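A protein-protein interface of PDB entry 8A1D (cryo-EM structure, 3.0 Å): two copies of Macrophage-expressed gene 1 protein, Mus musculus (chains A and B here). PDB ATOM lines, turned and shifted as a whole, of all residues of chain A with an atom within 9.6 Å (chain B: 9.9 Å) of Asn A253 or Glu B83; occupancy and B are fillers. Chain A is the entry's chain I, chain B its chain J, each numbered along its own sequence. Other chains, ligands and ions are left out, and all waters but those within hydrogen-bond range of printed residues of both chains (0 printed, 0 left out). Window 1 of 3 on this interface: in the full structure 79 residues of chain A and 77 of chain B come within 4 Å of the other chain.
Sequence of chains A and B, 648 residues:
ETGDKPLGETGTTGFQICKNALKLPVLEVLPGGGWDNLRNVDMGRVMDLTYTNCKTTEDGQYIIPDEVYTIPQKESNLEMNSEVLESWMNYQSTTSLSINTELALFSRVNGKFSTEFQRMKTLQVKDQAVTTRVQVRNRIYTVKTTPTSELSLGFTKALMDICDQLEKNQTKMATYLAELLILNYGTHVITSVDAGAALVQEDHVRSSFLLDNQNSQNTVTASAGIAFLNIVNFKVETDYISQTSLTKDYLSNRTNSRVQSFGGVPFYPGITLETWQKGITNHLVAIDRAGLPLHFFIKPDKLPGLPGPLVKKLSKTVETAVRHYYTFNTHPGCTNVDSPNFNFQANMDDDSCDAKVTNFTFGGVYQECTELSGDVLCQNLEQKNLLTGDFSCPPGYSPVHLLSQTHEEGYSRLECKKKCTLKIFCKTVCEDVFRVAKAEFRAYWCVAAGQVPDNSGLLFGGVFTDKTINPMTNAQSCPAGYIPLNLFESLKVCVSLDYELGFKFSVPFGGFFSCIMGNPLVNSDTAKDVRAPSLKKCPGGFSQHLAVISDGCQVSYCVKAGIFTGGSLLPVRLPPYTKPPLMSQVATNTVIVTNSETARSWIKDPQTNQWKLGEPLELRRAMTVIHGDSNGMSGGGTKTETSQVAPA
Of the printed residues of chain B, Asn A253 touches Glu B83 (3.2 Å) and Val B84 (2.8 Å). Printed residues of chain A within 4 Å of Glu B83: Asn A253. No residue of chain A comes within 4 Å of Val B130. No residue of chain A comes within 4 Å of Thr B131. Printed residues of chain A within 4 Å of Ser B82: Arg A254 (3.5 Å) and Thr A255 (2.9 Å). Printed residues of chain B within 4 Å of Tyr A250: Glu B86 (3.3 Å) and Ser B87 (3.9 Å). Of the printed residues of chain A, Ser B87 touches Tyr A250. Of the printed residues of chain A, Met B80 touches Thr A255 (3.4 Å) and Asn A256 (3.2 Å). Val B205 touches none of the printed residues of chain A. Arg A206 touches none of the printed residues of chain B. The nearest printed residue of chain A that does not touch Glu B86 is Ser A252 (5.0 Å).
The backbone carbonyl oxygen (O) of Glu B86 sits at hydrogen-bond distance from the backbone NH (N) of Leu A251, at 2.8 Å. The backbone NH (N) of Ser B82 is in hydrogen-bond range of the backbone carbonyl oxygen (O) of Thr A255, 2.9 Å away. The backbone carbonyl oxygen of Val B84 lies within hydrogen-bond range of the backbone NH of Asn A253, 2.8 Å away. O of Thr A255 sits close to O of Met B80, 3.4 Å away.
The backbone NH (N) of Ala B129 is in hydrogen-bond range of the backbone carbonyl oxygen (O) of Leu B85, at 2.9 Å. O of Ser A252 sits at hydrogen-bond distance from N of Ser A208, at 2.9 Å. N of Glu B83 sits at hydrogen-bond distance from O of Thr B131 (2.9 Å). The backbone carbonyl oxygen of Asn A256 is in hydrogen-bond range of the backbone NH of His A204. OG of Ser A207 sits at hydrogen-bond distance from OD1 of Asn A253 (3.2 Å). The backbone carbonyl oxygen (O) of Arg A254 is in hydrogen-bond range of the backbone NH (N) of Arg A206 (2.9 Å).
Positions printed for both chains: 128, 129, 204, 205 and 206. Of the 15 pairs that touch across the chains among the printed residues, none has its exchanged pair printed and touching as well.
Printed residues of chain A that touch a printed residue of chain B: Tyr A250, Leu A251, Ser A252, Asn A253, Arg A254, Thr A255 and Asn A256. Hydrophobic or aromatic side chains of chain A that line the printed part of chain B: Tyr A250 and Leu A251. Among the printed residues, 15 pairs touch across the chains. Among the printed residues, no Asp or Glu carboxylate lies within 4 Å of a Lys or Arg side-chain nitrogen of the other chain.
Glu B86 touches Tyr A250 (O to CA, 3.3 Å). O of Val B84 touches O of Leu A251 (3.8 Å). Leu B85 touches Leu A251. Val B84 touches Ser A252. Ser A252 touches Leu B85 (OG to CD2, 3.6 Å). Asn A253 touches Glu B83. Arg A254 touches Ser B82 (CA to O, 3.5 Å). Asn B81 touches Thr A255. Asn A256 touches Met B80 (CA to O, 3.2 Å). OD1 of Asn A256 touches ND2 of Asn B81, at 3.6 Å.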
ATOM      1  N   LYS A 126       7.340  -3.303  13.873  1.00  0.00           N
ATOM      2  CA  LYS A 126       6.315  -4.207  14.369  1.00  0.00           C
ATOM      3  C   LYS A 126       6.888  -5.608  14.426  1.00  0.00           C
ATOM      4  O   LYS A 126       7.337  -6.132  13.409  1.00  0.00           O
ATOM      5  CB  LYS A 126       5.076  -4.167  13.481  1.00  0.00           C
ATOM      6  CG  LYS A 126       3.907  -4.894  14.070  1.00  0.00           C
ATOM      7  CD  LYS A 126       2.665  -4.671  13.249  1.00  0.00           C
ATOM      8  CE  LYS A 126       1.452  -5.274  13.932  1.00  0.00           C
ATOM      9  NZ  LYS A 126       0.210  -5.025  13.155  1.00  0.00           N
ATOM     10  N   ASP A 127       6.885  -6.209  15.606  1.00  0.00           N
ATOM     11  CA  ASP A 127       7.398  -7.554  15.800  1.00  0.00           C
ATOM     12  C   ASP A 127       6.311  -8.448  16.356  1.00  0.00           C
ATOM     13  O   ASP A 127       5.568  -8.049  17.250  1.00  0.00           O
ATOM     14  CB  ASP A 127       8.568  -7.576  16.763  1.00  0.00           C
ATOM     15  CG  ASP A 127       9.715  -6.754  16.283  1.00  0.00           C
ATOM     16  OD1 ASP A 127       9.597  -6.162  15.197  1.00  0.00           O
ATOM     17  OD2 ASP A 127      10.740  -6.705  16.989  1.00  0.00           O
ATOM     18  N   GLN A 128       6.237  -9.663  15.835  1.00  0.00           N
ATOM     19  CA  GLN A 128       5.365 -10.684  16.387  1.00  0.00           C
ATOM     20  C   GLN A 128       6.172 -11.948  16.569  1.00  0.00           C
ATOM     21  O   GLN A 128       6.963 -12.306  15.697  1.00  0.00           O
ATOM     22  CB  GLN A 128       4.182 -10.976  15.478  1.00  0.00           C
ATOM     23  CG  GLN A 128       3.309  -9.802  15.218  1.00  0.00           C
ATOM     24  CD  GLN A 128       2.034 -10.212  14.541  1.00  0.00           C
ATOM     25  OE1 GLN A 128       1.808 -11.396  14.301  1.00  0.00           O
ATOM     26  NE2 GLN A 128       1.193  -9.240  14.217  1.00  0.00           N
ATOM     27  N   ALA A 129       5.961 -12.623  17.684  1.00  0.00           N
ATOM     28  CA  ALA A 129       6.583 -13.913  17.933  1.00  0.00           C
ATOM     29  C   ALA A 129       5.527 -14.798  18.566  1.00  0.00           C
ATOM     30  O   ALA A 129       5.136 -14.577  19.713  1.00  0.00           O
ATOM     31  CB  ALA A 129       7.807 -13.781  18.829  1.00  0.00           C
ATOM     32  N   HIS A 204       6.685 -22.060  15.611  1.00  0.00           N
ATOM     33  CA  HIS A 204       7.234 -20.731  15.831  1.00  0.00           C
ATOM     34  C   HIS A 204       6.879 -19.866  14.643  1.00  0.00           C
ATOM     35  O   HIS A 204       6.985 -20.312  13.503  1.00  0.00           O
ATOM     36  CB  HIS A 204       8.746 -20.765  15.996  1.00  0.00           C
ATOM     37  CG  HIS A 204       9.212 -21.571  17.158  1.00  0.00           C
ATOM     38  ND1 HIS A 204       9.041 -22.934  17.233  1.00  0.00           N
ATOM     39  CD2 HIS A 204       9.885 -21.212  18.274  1.00  0.00           C
ATOM     40  CE1 HIS A 204       9.570 -23.379  18.358  1.00  0.00           C
ATOM     41  NE2 HIS A 204      10.087 -22.354  19.008  1.00  0.00           N
ATOM     42  N   VAL A 205       6.465 -18.638  14.907  1.00  0.00           N
ATOM     43  CA  VAL A 205       6.251 -17.640  13.873  1.00  0.00           C
ATOM     44  C   VAL A 205       6.923 -16.365  14.332  1.00  0.00           C
ATOM     45  O   VAL A 205       6.718 -15.931  15.467  1.00  0.00           O
ATOM     46  CB  VAL A 205       4.763 -17.401  13.605  1.00  0.00           C
ATOM     47  CG1 VAL A 205       4.604 -16.320  12.584  1.00  0.00           C
ATOM     48  CG2 VAL A 205       4.118 -18.660  13.125  1.00  0.00           C
ATOM     49  N   ARG A 206       7.738 -15.775  13.470  1.00  0.00           N
ATOM     50  CA  ARG A 206       8.356 -14.489  13.750  1.00  0.00           C
ATOM     51  C   ARG A 206       8.110 -13.569  12.572  1.00  0.00           C
ATOM     52  O   ARG A 206       8.465 -13.903  11.440  1.00  0.00           O
ATOM     53  CB  ARG A 206       9.850 -14.631  14.009  1.00  0.00           C
ATOM     54  CG  ARG A 206      10.168 -15.501  15.186  1.00  0.00           C
ATOM     55  CD  ARG A 206      11.657 -15.569  15.433  1.00  0.00           C
ATOM     56  NE  ARG A 206      11.970 -16.435  16.563  1.00  0.00           N
ATOM     57  CZ  ARG A 206      13.194 -16.673  17.011  1.00  0.00           C
ATOM     58  NH1 ARG A 206      14.256 -16.119  16.448  1.00  0.00           N
ATOM     59  NH2 ARG A 206      13.359 -17.485  18.051  1.00  0.00           N
ATOM     60  N   SER A 207       7.514 -12.419  12.834  1.00  0.00           N
ATOM     61  CA  SER A 207       7.284 -11.409  11.816  1.00  0.00           C
ATOM     62  C   SER A 207       7.942 -10.117  12.254  1.00  0.00           C
ATOM     63  O   SER A 207       7.783  -9.697  13.399  1.00  0.00           O
ATOM     64  CB  SER A 207       5.797 -11.177  11.580  1.00  0.00           C
ATOM     65  OG  SER A 207       5.145 -12.380  11.242  1.00  0.00           O
ATOM     66  N   SER A 208       8.680  -9.499  11.349  1.00  0.00           N
ATOM     67  CA  SER A 208       9.276  -8.197  11.582  1.00  0.00           C
ATOM     68  C   SER A 208       8.906  -7.294  10.426  1.00  0.00           C
ATOM     69  O   SER A 208       9.056  -7.676   9.265  1.00  0.00           O
ATOM     70  CB  SER A 208      10.790  -8.288  11.712  1.00  0.00           C
ATOM     71  OG  SER A 208      11.143  -9.157  12.767  1.00  0.00           O
ATOM     72  N   PHE A 209       8.414  -6.112  10.740  1.00  0.00           N
ATOM     73  CA  PHE A 209       8.042  -5.142   9.729  1.00  0.00           C
ATOM     74  C   PHE A 209       8.653  -3.809  10.099  1.00  0.00           C
ATOM     75  O   PHE A 209       8.497  -3.347  11.228  1.00  0.00           O
ATOM     76  CB  PHE A 209       6.534  -5.029   9.618  1.00  0.00           C
ATOM     77  CG  PHE A 209       6.086  -3.904   8.766  1.00  0.00           C
ATOM     78  CD1 PHE A 209       6.224  -3.959   7.399  1.00  0.00           C
ATOM     79  CD2 PHE A 209       5.508  -2.792   9.331  1.00  0.00           C
ATOM     80  CE1 PHE A 209       5.802  -2.919   6.612  1.00  0.00           C
ATOM     81  CE2 PHE A 209       5.086  -1.750   8.550  1.00  0.00           C
ATOM     82  CZ  PHE A 209       5.232  -1.813   7.189  1.00  0.00           C
ATOM     83  N   TYR A 250      10.286  -3.073   4.827  1.00  0.00           N
ATOM     84  CA  TYR A 250      11.035  -4.304   4.985  1.00  0.00           C
ATOM     85  C   TYR A 250      10.172  -5.263   5.779  1.00  0.00           C
ATOM     86  O   TYR A 250       9.740  -4.932   6.881  1.00  0.00           O
ATOM     87  CB  TYR A 250      12.358  -4.050   5.696  1.00  0.00           C
ATOM     88  CG  TYR A 250      13.206  -5.278   5.860  1.00  0.00           C
ATOM     89  CD1 TYR A 250      13.996  -5.735   4.818  1.00  0.00           C
ATOM     90  CD2 TYR A 250      13.221  -5.986   7.049  1.00  0.00           C
ATOM     91  CE1 TYR A 250      14.781  -6.860   4.956  1.00  0.00           C
ATOM     92  CE2 TYR A 250      14.005  -7.113   7.198  1.00  0.00           C
ATOM     93  CZ  TYR A 250      14.782  -7.544   6.146  1.00  0.00           C
ATOM     94  OH  TYR A 250      15.564  -8.665   6.284  1.00  0.00           O
ATOM     95  N   LEU A 251       9.917  -6.434   5.227  1.00  0.00           N
ATOM     96  CA  LEU A 251       9.060  -7.413   5.867  1.00  0.00           C
ATOM     97  C   LEU A 251       9.814  -8.719   5.981  1.00  0.00           C
ATOM     98  O   LEU A 251      10.633  -9.042   5.123  1.00  0.00           O
ATOM     99  CB  LEU A 251       7.780  -7.612   5.083  1.00  0.00           C
ATOM    100  CG  LEU A 251       6.760  -8.576   5.666  1.00  0.00           C
ATOM    101  CD1 LEU A 251       6.316  -8.087   7.008  1.00  0.00           C
ATOM    102  CD2 LEU A 251       5.579  -8.683   4.736  1.00  0.00           C
ATOM    103  N   SER A 252       9.556  -9.461   7.047  1.00  0.00           N
ATOM    104  CA  SER A 252      10.285 -10.701   7.277  1.00  0.00           C
ATOM    105  C   SER A 252       9.387 -11.655   8.042  1.00  0.00           C
ATOM    106  O   SER A 252       9.011 -11.368   9.176  1.00  0.00           O
ATOM    107  CB  SER A 252      11.571 -10.432   8.042  1.00  0.00           C
ATOM    108  OG  SER A 252      12.221 -11.640   8.367  1.00  0.00           O
ATOM    109  N   ASN A 253       9.045 -12.777   7.428  1.00  0.00           N
ATOM    110  CA  ASN A 253       8.291 -13.839   8.071  1.00  0.00           C
ATOM    111  C   ASN A 253       9.167 -15.070   8.194  1.00  0.00           C
ATOM    112  O   ASN A 253       9.940 -15.376   7.290  1.00  0.00           O
ATOM    113  CB  ASN A 253       7.056 -14.201   7.269  1.00  0.00           C
ATOM    114  CG  ASN A 253       5.882 -13.343   7.591  1.00  0.00           C
ATOM    115  OD1 ASN A 253       6.014 -12.269   8.162  1.00  0.00           O
ATOM    116  ND2 ASN A 253       4.710 -13.818   7.216  1.00  0.00           N
ATOM    117  N   ARG A 254       9.043 -15.780   9.303  1.00  0.00           N
ATOM    118  CA  ARG A 254       9.787 -17.019   9.501  1.00  0.00           C
ATOM    119  C   ARG A 254       8.929 -17.946  10.340  1.00  0.00           C
ATOM    120  O   ARG A 254       8.690 -17.664  11.512  1.00  0.00           O
ATOM    121  CB  ARG A 254      11.122 -16.760  10.187  1.00  0.00           C
ATOM    122  CG  ARG A 254      12.142 -16.059   9.341  1.00  0.00           C
ATOM    123  CD  ARG A 254      13.433 -15.859  10.100  1.00  0.00           C
ATOM    124  NE  ARG A 254      14.072 -17.125  10.437  1.00  0.00           N
ATOM    125  CZ  ARG A 254      14.098 -17.652  11.653  1.00  0.00           C
ATOM    126  NH1 ARG A 254      13.544 -17.038  12.685  1.00  0.00           N
ATOM    127  NH2 ARG A 254      14.701 -18.823  11.840  1.00  0.00           N
ATOM    128  N   THR A 255       8.469 -19.045   9.757  1.00  0.00           N
ATOM    129  CA  THR A 255       7.623 -19.998  10.461  1.00  0.00           C
ATOM    130  C   THR A 255       8.301 -21.355  10.451  1.00  0.00           C
ATOM    131  O   THR A 255       8.742 -21.821   9.401  1.00  0.00           O
ATOM    132  CB  THR A 255       6.249 -20.100   9.814  1.00  0.00           C
ATOM    133  OG1 THR A 255       6.335 -20.937   8.662  1.00  0.00           O
ATOM    134  CG2 THR A 255       5.778 -18.737   9.377  1.00  0.00           C
ATOM    135  N   ASN A 256       8.384 -21.985  11.615  1.00  0.00           N
ATOM    136  CA  ASN A 256       8.926 -23.330  11.737  1.00  0.00           C
ATOM    137  C   ASN A 256       7.899 -24.199  12.428  1.00  0.00           C
ATOM    138  O   ASN A 256       7.443 -23.869  13.520  1.00  0.00           O
ATOM    139  CB  ASN A 256      10.223 -23.342  12.534  1.00  0.00           C
ATOM    140  CG  ASN A 256      11.169 -22.284  12.091  1.00  0.00           C
ATOM    141  OD1 ASN A 256      11.161 -21.881  10.935  1.00  0.00           O
ATOM    142  ND2 ASN A 256      12.003 -21.818  13.005  1.00  0.00           N
ATOM    143  N   MET B  80       8.393 -28.071   8.749  1.00  0.00           N
ATOM    144  CA  MET B  80       7.938 -27.082   7.791  1.00  0.00           C
ATOM    145  C   MET B  80       8.646 -25.780   8.106  1.00  0.00           C
ATOM    146  O   MET B  80       8.500 -25.250   9.208  1.00  0.00           O
ATOM    147  CB  MET B  80       6.425 -26.912   7.861  1.00  0.00           C
ATOM    148  CG  MET B  80       5.662 -28.051   7.242  1.00  0.00           C
ATOM    149  SD  MET B  80       3.882 -27.842   7.360  1.00  0.00           S
ATOM    150  CE  MET B  80       3.559 -28.683   8.905  1.00  0.00           C
ATOM    151  N   ASN B  81       9.415 -25.272   7.156  1.00  0.00           N
ATOM    152  CA  ASN B  81      10.038 -23.964   7.286  1.00  0.00           C
ATOM    153  C   ASN B  81       9.491 -23.093   6.181  1.00  0.00           C
ATOM    154  O   ASN B  81       9.343 -23.550   5.048  1.00  0.00           O
ATOM    155  CB  ASN B  81      11.555 -24.036   7.195  1.00  0.00           C
ATOM    156  CG  ASN B  81      12.134 -25.077   8.096  1.00  0.00           C
ATOM    157  OD1 ASN B  81      12.883 -25.942   7.660  1.00  0.00           O
ATOM    158  ND2 ASN B  81      11.785 -25.014   9.366  1.00  0.00           N
ATOM    159  N   SER B  82       9.171 -21.858   6.509  1.00  0.00           N
ATOM    160  CA  SER B  82       8.774 -20.870   5.528  1.00  0.00           C
ATOM    161  C   SER B  82       9.528 -19.597   5.840  1.00  0.00           C
ATOM    162  O   SER B  82       9.929 -19.380   6.983  1.00  0.00           O
ATOM    163  CB  SER B  82       7.274 -20.622   5.553  1.00  0.00           C
ATOM    164  OG  SER B  82       6.931 -19.615   4.627  1.00  0.00           O
ATOM    165  N   GLU B  83       9.754 -18.776   4.825  1.00  0.00           N
ATOM    166  CA  GLU B  83      10.458 -17.522   5.029  1.00  0.00           C
ATOM    167  C   GLU B  83      10.094 -16.563   3.916  1.00  0.00           C
ATOM    168  O   GLU B  83      10.378 -16.832   2.750  1.00  0.00           O
ATOM    169  CB  GLU B  83      11.962 -17.748   5.080  1.00  0.00           C
ATOM    170  CG  GLU B  83      12.735 -16.509   5.398  1.00  0.00           C
ATOM    171  CD  GLU B  83      14.146 -16.824   5.816  1.00  0.00           C
ATOM    172  OE1 GLU B  83      14.493 -18.021   5.843  1.00  0.00           O
ATOM    173  OE2 GLU B  83      14.900 -15.883   6.141  1.00  0.00           O
ATOM    174  N   VAL B  84       9.474 -15.448   4.274  1.00  0.00           N
ATOM    175  CA  VAL B  84       9.063 -14.433   3.320  1.00  0.00           C
ATOM    176  C   VAL B  84       9.826 -13.161   3.630  1.00  0.00           C
ATOM    177  O   VAL B  84       9.799 -12.685   4.767  1.00  0.00           O
ATOM    178  CB  VAL B  84       7.552 -14.175   3.387  1.00  0.00           C
ATOM    179  CG1 VAL B  84       7.167 -13.128   2.389  1.00  0.00           C
ATOM    180  CG2 VAL B  84       6.799 -15.447   3.141  1.00  0.00           C
ATOM    181  N   LEU B  85      10.507 -12.617   2.631  1.00  0.00           N
ATOM    182  CA  LEU B  85      11.174 -11.330   2.761  1.00  0.00           C
ATOM    183  C   LEU B  85      10.614 -10.406   1.700  1.00  0.00           C
ATOM    184  O   LEU B  85      10.492 -10.800   0.542  1.00  0.00           O
ATOM    185  CB  LEU B  85      12.682 -11.460   2.600  1.00  0.00           C
ATOM    186  CG  LEU B  85      13.334 -12.539   3.447  1.00  0.00           C
ATOM    187  CD1 LEU B  85      14.824 -12.543   3.220  1.00  0.00           C
ATOM    188  CD2 LEU B  85      13.022 -12.321   4.898  1.00  0.00           C
ATOM    189  N   GLU B  86      10.256  -9.196   2.088  1.00  0.00           N
ATOM    190  CA  GLU B  86       9.802  -8.205   1.132  1.00  0.00           C
ATOM    191  C   GLU B  86      10.490  -6.884   1.400  1.00  0.00           C
ATOM    192  O   GLU B  86      10.656  -6.482   2.551  1.00  0.00           O
ATOM    193  CB  GLU B  86       8.298  -8.024   1.187  1.00  0.00           C
ATOM    194  CG  GLU B  86       7.538  -9.265   0.826  1.00  0.00           C
ATOM    195  CD  GLU B  86       6.065  -9.005   0.671  1.00  0.00           C
ATOM    196  OE1 GLU B  86       5.661  -7.831   0.773  1.00  0.00           O
ATOM    197  OE2 GLU B  86       5.308  -9.970   0.446  1.00  0.00           O
ATOM    198  N   SER B  87      10.894  -6.221   0.329  1.00  0.00           N
ATOM    199  CA  SER B  87      11.483  -4.894   0.406  1.00  0.00           C
ATOM    200  C   SER B  87      10.734  -3.996  -0.552  1.00  0.00           C
ATOM    201  O   SER B  87      10.497  -4.377  -1.696  1.00  0.00           O
ATOM    202  CB  SER B  87      12.966  -4.915   0.052  1.00  0.00           C
ATOM    203  OG  SER B  87      13.665  -5.801   0.899  1.00  0.00           O
ATOM    204  N   GLN B 128      10.427  -9.564  -3.509  1.00  0.00           N
ATOM    205  CA  GLN B 128       9.839 -10.599  -2.680  1.00  0.00           C
ATOM    206  C   GLN B 128      10.660 -11.857  -2.838  1.00  0.00           C
ATOM    207  O   GLN B 128      11.004 -12.234  -3.958  1.00  0.00           O
ATOM    208  CB  GLN B 128       8.396 -10.885  -3.066  1.00  0.00           C
ATOM    209  CG  GLN B 128       7.492  -9.710  -2.932  1.00  0.00           C
ATOM    210  CD  GLN B 128       6.057 -10.104  -3.119  1.00  0.00           C
ATOM    211  OE1 GLN B 128       5.757 -11.274  -3.346  1.00  0.00           O
ATOM    212  NE2 GLN B 128       5.157  -9.134  -3.046  1.00  0.00           N
ATOM    213  N   ALA B 129      10.965 -12.502  -1.726  1.00  0.00           N
ATOM    214  CA  ALA B 129      11.672 -13.771  -1.726  1.00  0.00           C
ATOM    215  C   ALA B 129      10.937 -14.699  -0.779  1.00  0.00           C
ATOM    216  O   ALA B 129      10.919 -14.468   0.430  1.00  0.00           O
ATOM    217  CB  ALA B 129      13.126 -13.598  -1.306  1.00  0.00           C
ATOM    218  N   VAL B 130      10.325 -15.737  -1.324  1.00  0.00           N
ATOM    219  CA  VAL B 130       9.587 -16.716  -0.544  1.00  0.00           C
ATOM    220  C   VAL B 130      10.317 -18.037  -0.639  1.00  0.00           C
ATOM    221  O   VAL B 130      10.616 -18.504  -1.739  1.00  0.00           O
ATOM    222  CB  VAL B 130       8.145 -16.863  -1.044  1.00  0.00           C
ATOM    223  CG1 VAL B 130       7.399 -17.826  -0.168  1.00  0.00           C
ATOM    224  CG2 VAL B 130       7.466 -15.526  -1.055  1.00  0.00           C
ATOM    225  N   THR B 131      10.605 -18.635   0.503  1.00  0.00           N
ATOM    226  CA  THR B 131      11.247 -19.934   0.559  1.00  0.00           C
ATOM    227  C   THR B 131      10.389 -20.841   1.414  1.00  0.00           C
ATOM    228  O   THR B 131       9.893 -20.422   2.460  1.00  0.00           O
ATOM    229  CB  THR B 131      12.650 -19.834   1.134  1.00  0.00           C
ATOM    230  OG1 THR B 131      13.429 -18.950   0.324  1.00  0.00           O
ATOM    231  CG2 THR B 131      13.304 -21.187   1.157  1.00  0.00           C
ATOM    232  N   THR B 132      10.191 -22.066   0.962  1.00  0.00           N
ATOM    233  CA  THR B 132       9.357 -23.025   1.665  1.00  0.00           C
ATOM    234  C   THR B 132      10.032 -24.379   1.606  1.00  0.00           C
ATOM    235  O   THR B 132      10.559 -24.761   0.563  1.00  0.00           O
ATOM    236  CB  THR B 132       7.967 -23.096   1.045  1.00  0.00           C
ATOM    237  OG1 THR B 132       7.367 -21.799   1.083  1.00  0.00           O
ATOM    238  CG2 THR B 132       7.100 -24.061   1.801  1.00  0.00           C
ATOM    239  N   ARG B 133      10.030 -25.098   2.717  1.00  0.00           N
ATOM    240  CA  ARG B 133      10.622 -26.421   2.770  1.00  0.00           C
ATOM    241  C   ARG B 133       9.766 -27.305   3.652  1.00  0.00           C
ATOM    242  O   ARG B 133       9.562 -27.000   4.826  1.00  0.00           O
ATOM    243  CB  ARG B 133      12.049 -26.362   3.296  1.00  0.00           C
ATOM    244  CG  ARG B 133      12.661 -27.712   3.490  1.00  0.00           C
ATOM    245  CD  ARG B 133      14.075 -27.594   3.980  1.00  0.00           C
ATOM    246  NE  ARG B 133      14.649 -28.903   4.253  1.00  0.00           N
ATOM    247  CZ  ARG B 133      15.267 -29.655   3.355  1.00  0.00           C
ATOM    248  NH1 ARG B 133      15.420 -29.254   2.105  1.00  0.00           N
ATOM    249  NH2 ARG B 133      15.748 -30.838   3.721  1.00  0.00           N
ATOM    250  N   VAL B 134       9.274 -28.397   3.089  1.00  0.00           N
ATOM    251  CA  VAL B 134       8.474 -29.374   3.810  1.00  0.00           C
ATOM    252  C   VAL B 134       9.241 -30.679   3.810  1.00  0.00           C
ATOM    253  O   VAL B 134       9.830 -31.051   2.795  1.00  0.00           O
ATOM    254  CB  VAL B 134       7.094 -29.552   3.169  1.00  0.00           C
ATOM    255  CG1 VAL B 134       6.313 -30.591   3.907  1.00  0.00           C
ATOM    256  CG2 VAL B 134       6.358 -28.248   3.172  1.00  0.00           C
ATOM    257  N   ASP B 203      10.646 -24.929  -2.295  1.00  0.00           N
ATOM    258  CA  ASP B 203       9.979 -23.960  -3.142  1.00  0.00           C
ATOM    259  C   ASP B 203      10.643 -22.607  -2.966  1.00  0.00           C
ATOM    260  O   ASP B 203      10.873 -22.173  -1.839  1.00  0.00           O
ATOM    261  CB  ASP B 203       8.504 -23.880  -2.791  1.00  0.00           C
ATOM    262  CG  ASP B 203       7.726 -23.089  -3.789  1.00  0.00           C
ATOM    263  OD1 ASP B 203       8.304 -22.749  -4.835  1.00  0.00           O
ATOM    264  OD2 ASP B 203       6.540 -22.808  -3.538  1.00  0.00           O
ATOM    265  N   HIS B 204      10.946 -21.946  -4.074  1.00  0.00           N
ATOM    266  CA  HIS B 204      11.527 -20.611  -4.060  1.00  0.00           C
ATOM    267  C   HIS B 204      10.740 -19.740  -5.017  1.00  0.00           C
ATOM    268  O   HIS B 204      10.391 -20.184  -6.110  1.00  0.00           O
ATOM    269  CB  HIS B 204      12.992 -20.632  -4.478  1.00  0.00           C
ATOM    270  CG  HIS B 204      13.885 -21.351  -3.524  1.00  0.00           C
ATOM    271  ND1 HIS B 204      13.786 -22.703  -3.291  1.00  0.00           N
ATOM    272  CD2 HIS B 204      14.918 -20.913  -2.770  1.00  0.00           C
ATOM    273  CE1 HIS B 204      14.709 -23.066  -2.420  1.00  0.00           C
ATOM    274  NE2 HIS B 204      15.411 -21.997  -2.088  1.00  0.00           N
ATOM    275  N   VAL B 205      10.461 -18.514  -4.610  1.00  0.00           N
ATOM    276  CA  VAL B 205       9.862 -17.512  -5.476  1.00  0.00           C
ATOM    277  C   VAL B 205      10.634 -16.221  -5.302  1.00  0.00           C
ATOM    278  O   VAL B 205      10.782 -15.735  -4.179  1.00  0.00           O
ATOM    279  CB  VAL B 205       8.377 -17.294  -5.161  1.00  0.00           C
ATOM    280  CG1 VAL B 205       7.838 -16.195  -6.027  1.00  0.00           C
ATOM    281  CG2 VAL B 205       7.601 -18.555  -5.393  1.00  0.00           C
ATOM    282  N   ARG B 206      11.125 -15.670  -6.404  1.00  0.00           N
ATOM    283  CA  ARG B 206      11.795 -14.380  -6.411  1.00  0.00           C
ATOM    284  C   ARG B 206      11.019 -13.461  -7.329  1.00  0.00           C
ATOM    285  O   ARG B 206      10.760 -13.812  -8.481  1.00  0.00           O
ATOM    286  CB  ARG B 206      13.238 -14.504  -6.890  1.00  0.00           C
ATOM    287  CG  ARG B 206      14.249 -14.488  -5.787  1.00  0.00           C
ATOM    288  CD  ARG B 206      14.641 -15.897  -5.429  1.00  0.00           C
ATOM    289  NE  ARG B 206      15.609 -15.938  -4.342  1.00  0.00           N
ATOM    290  CZ  ARG B 206      15.668 -16.905  -3.437  1.00  0.00           C
ATOM    291  NH1 ARG B 206      14.827 -17.924  -3.459  1.00  0.00           N
ATOM    292  NH2 ARG B 206      16.592 -16.844  -2.482  1.00  0.00           N
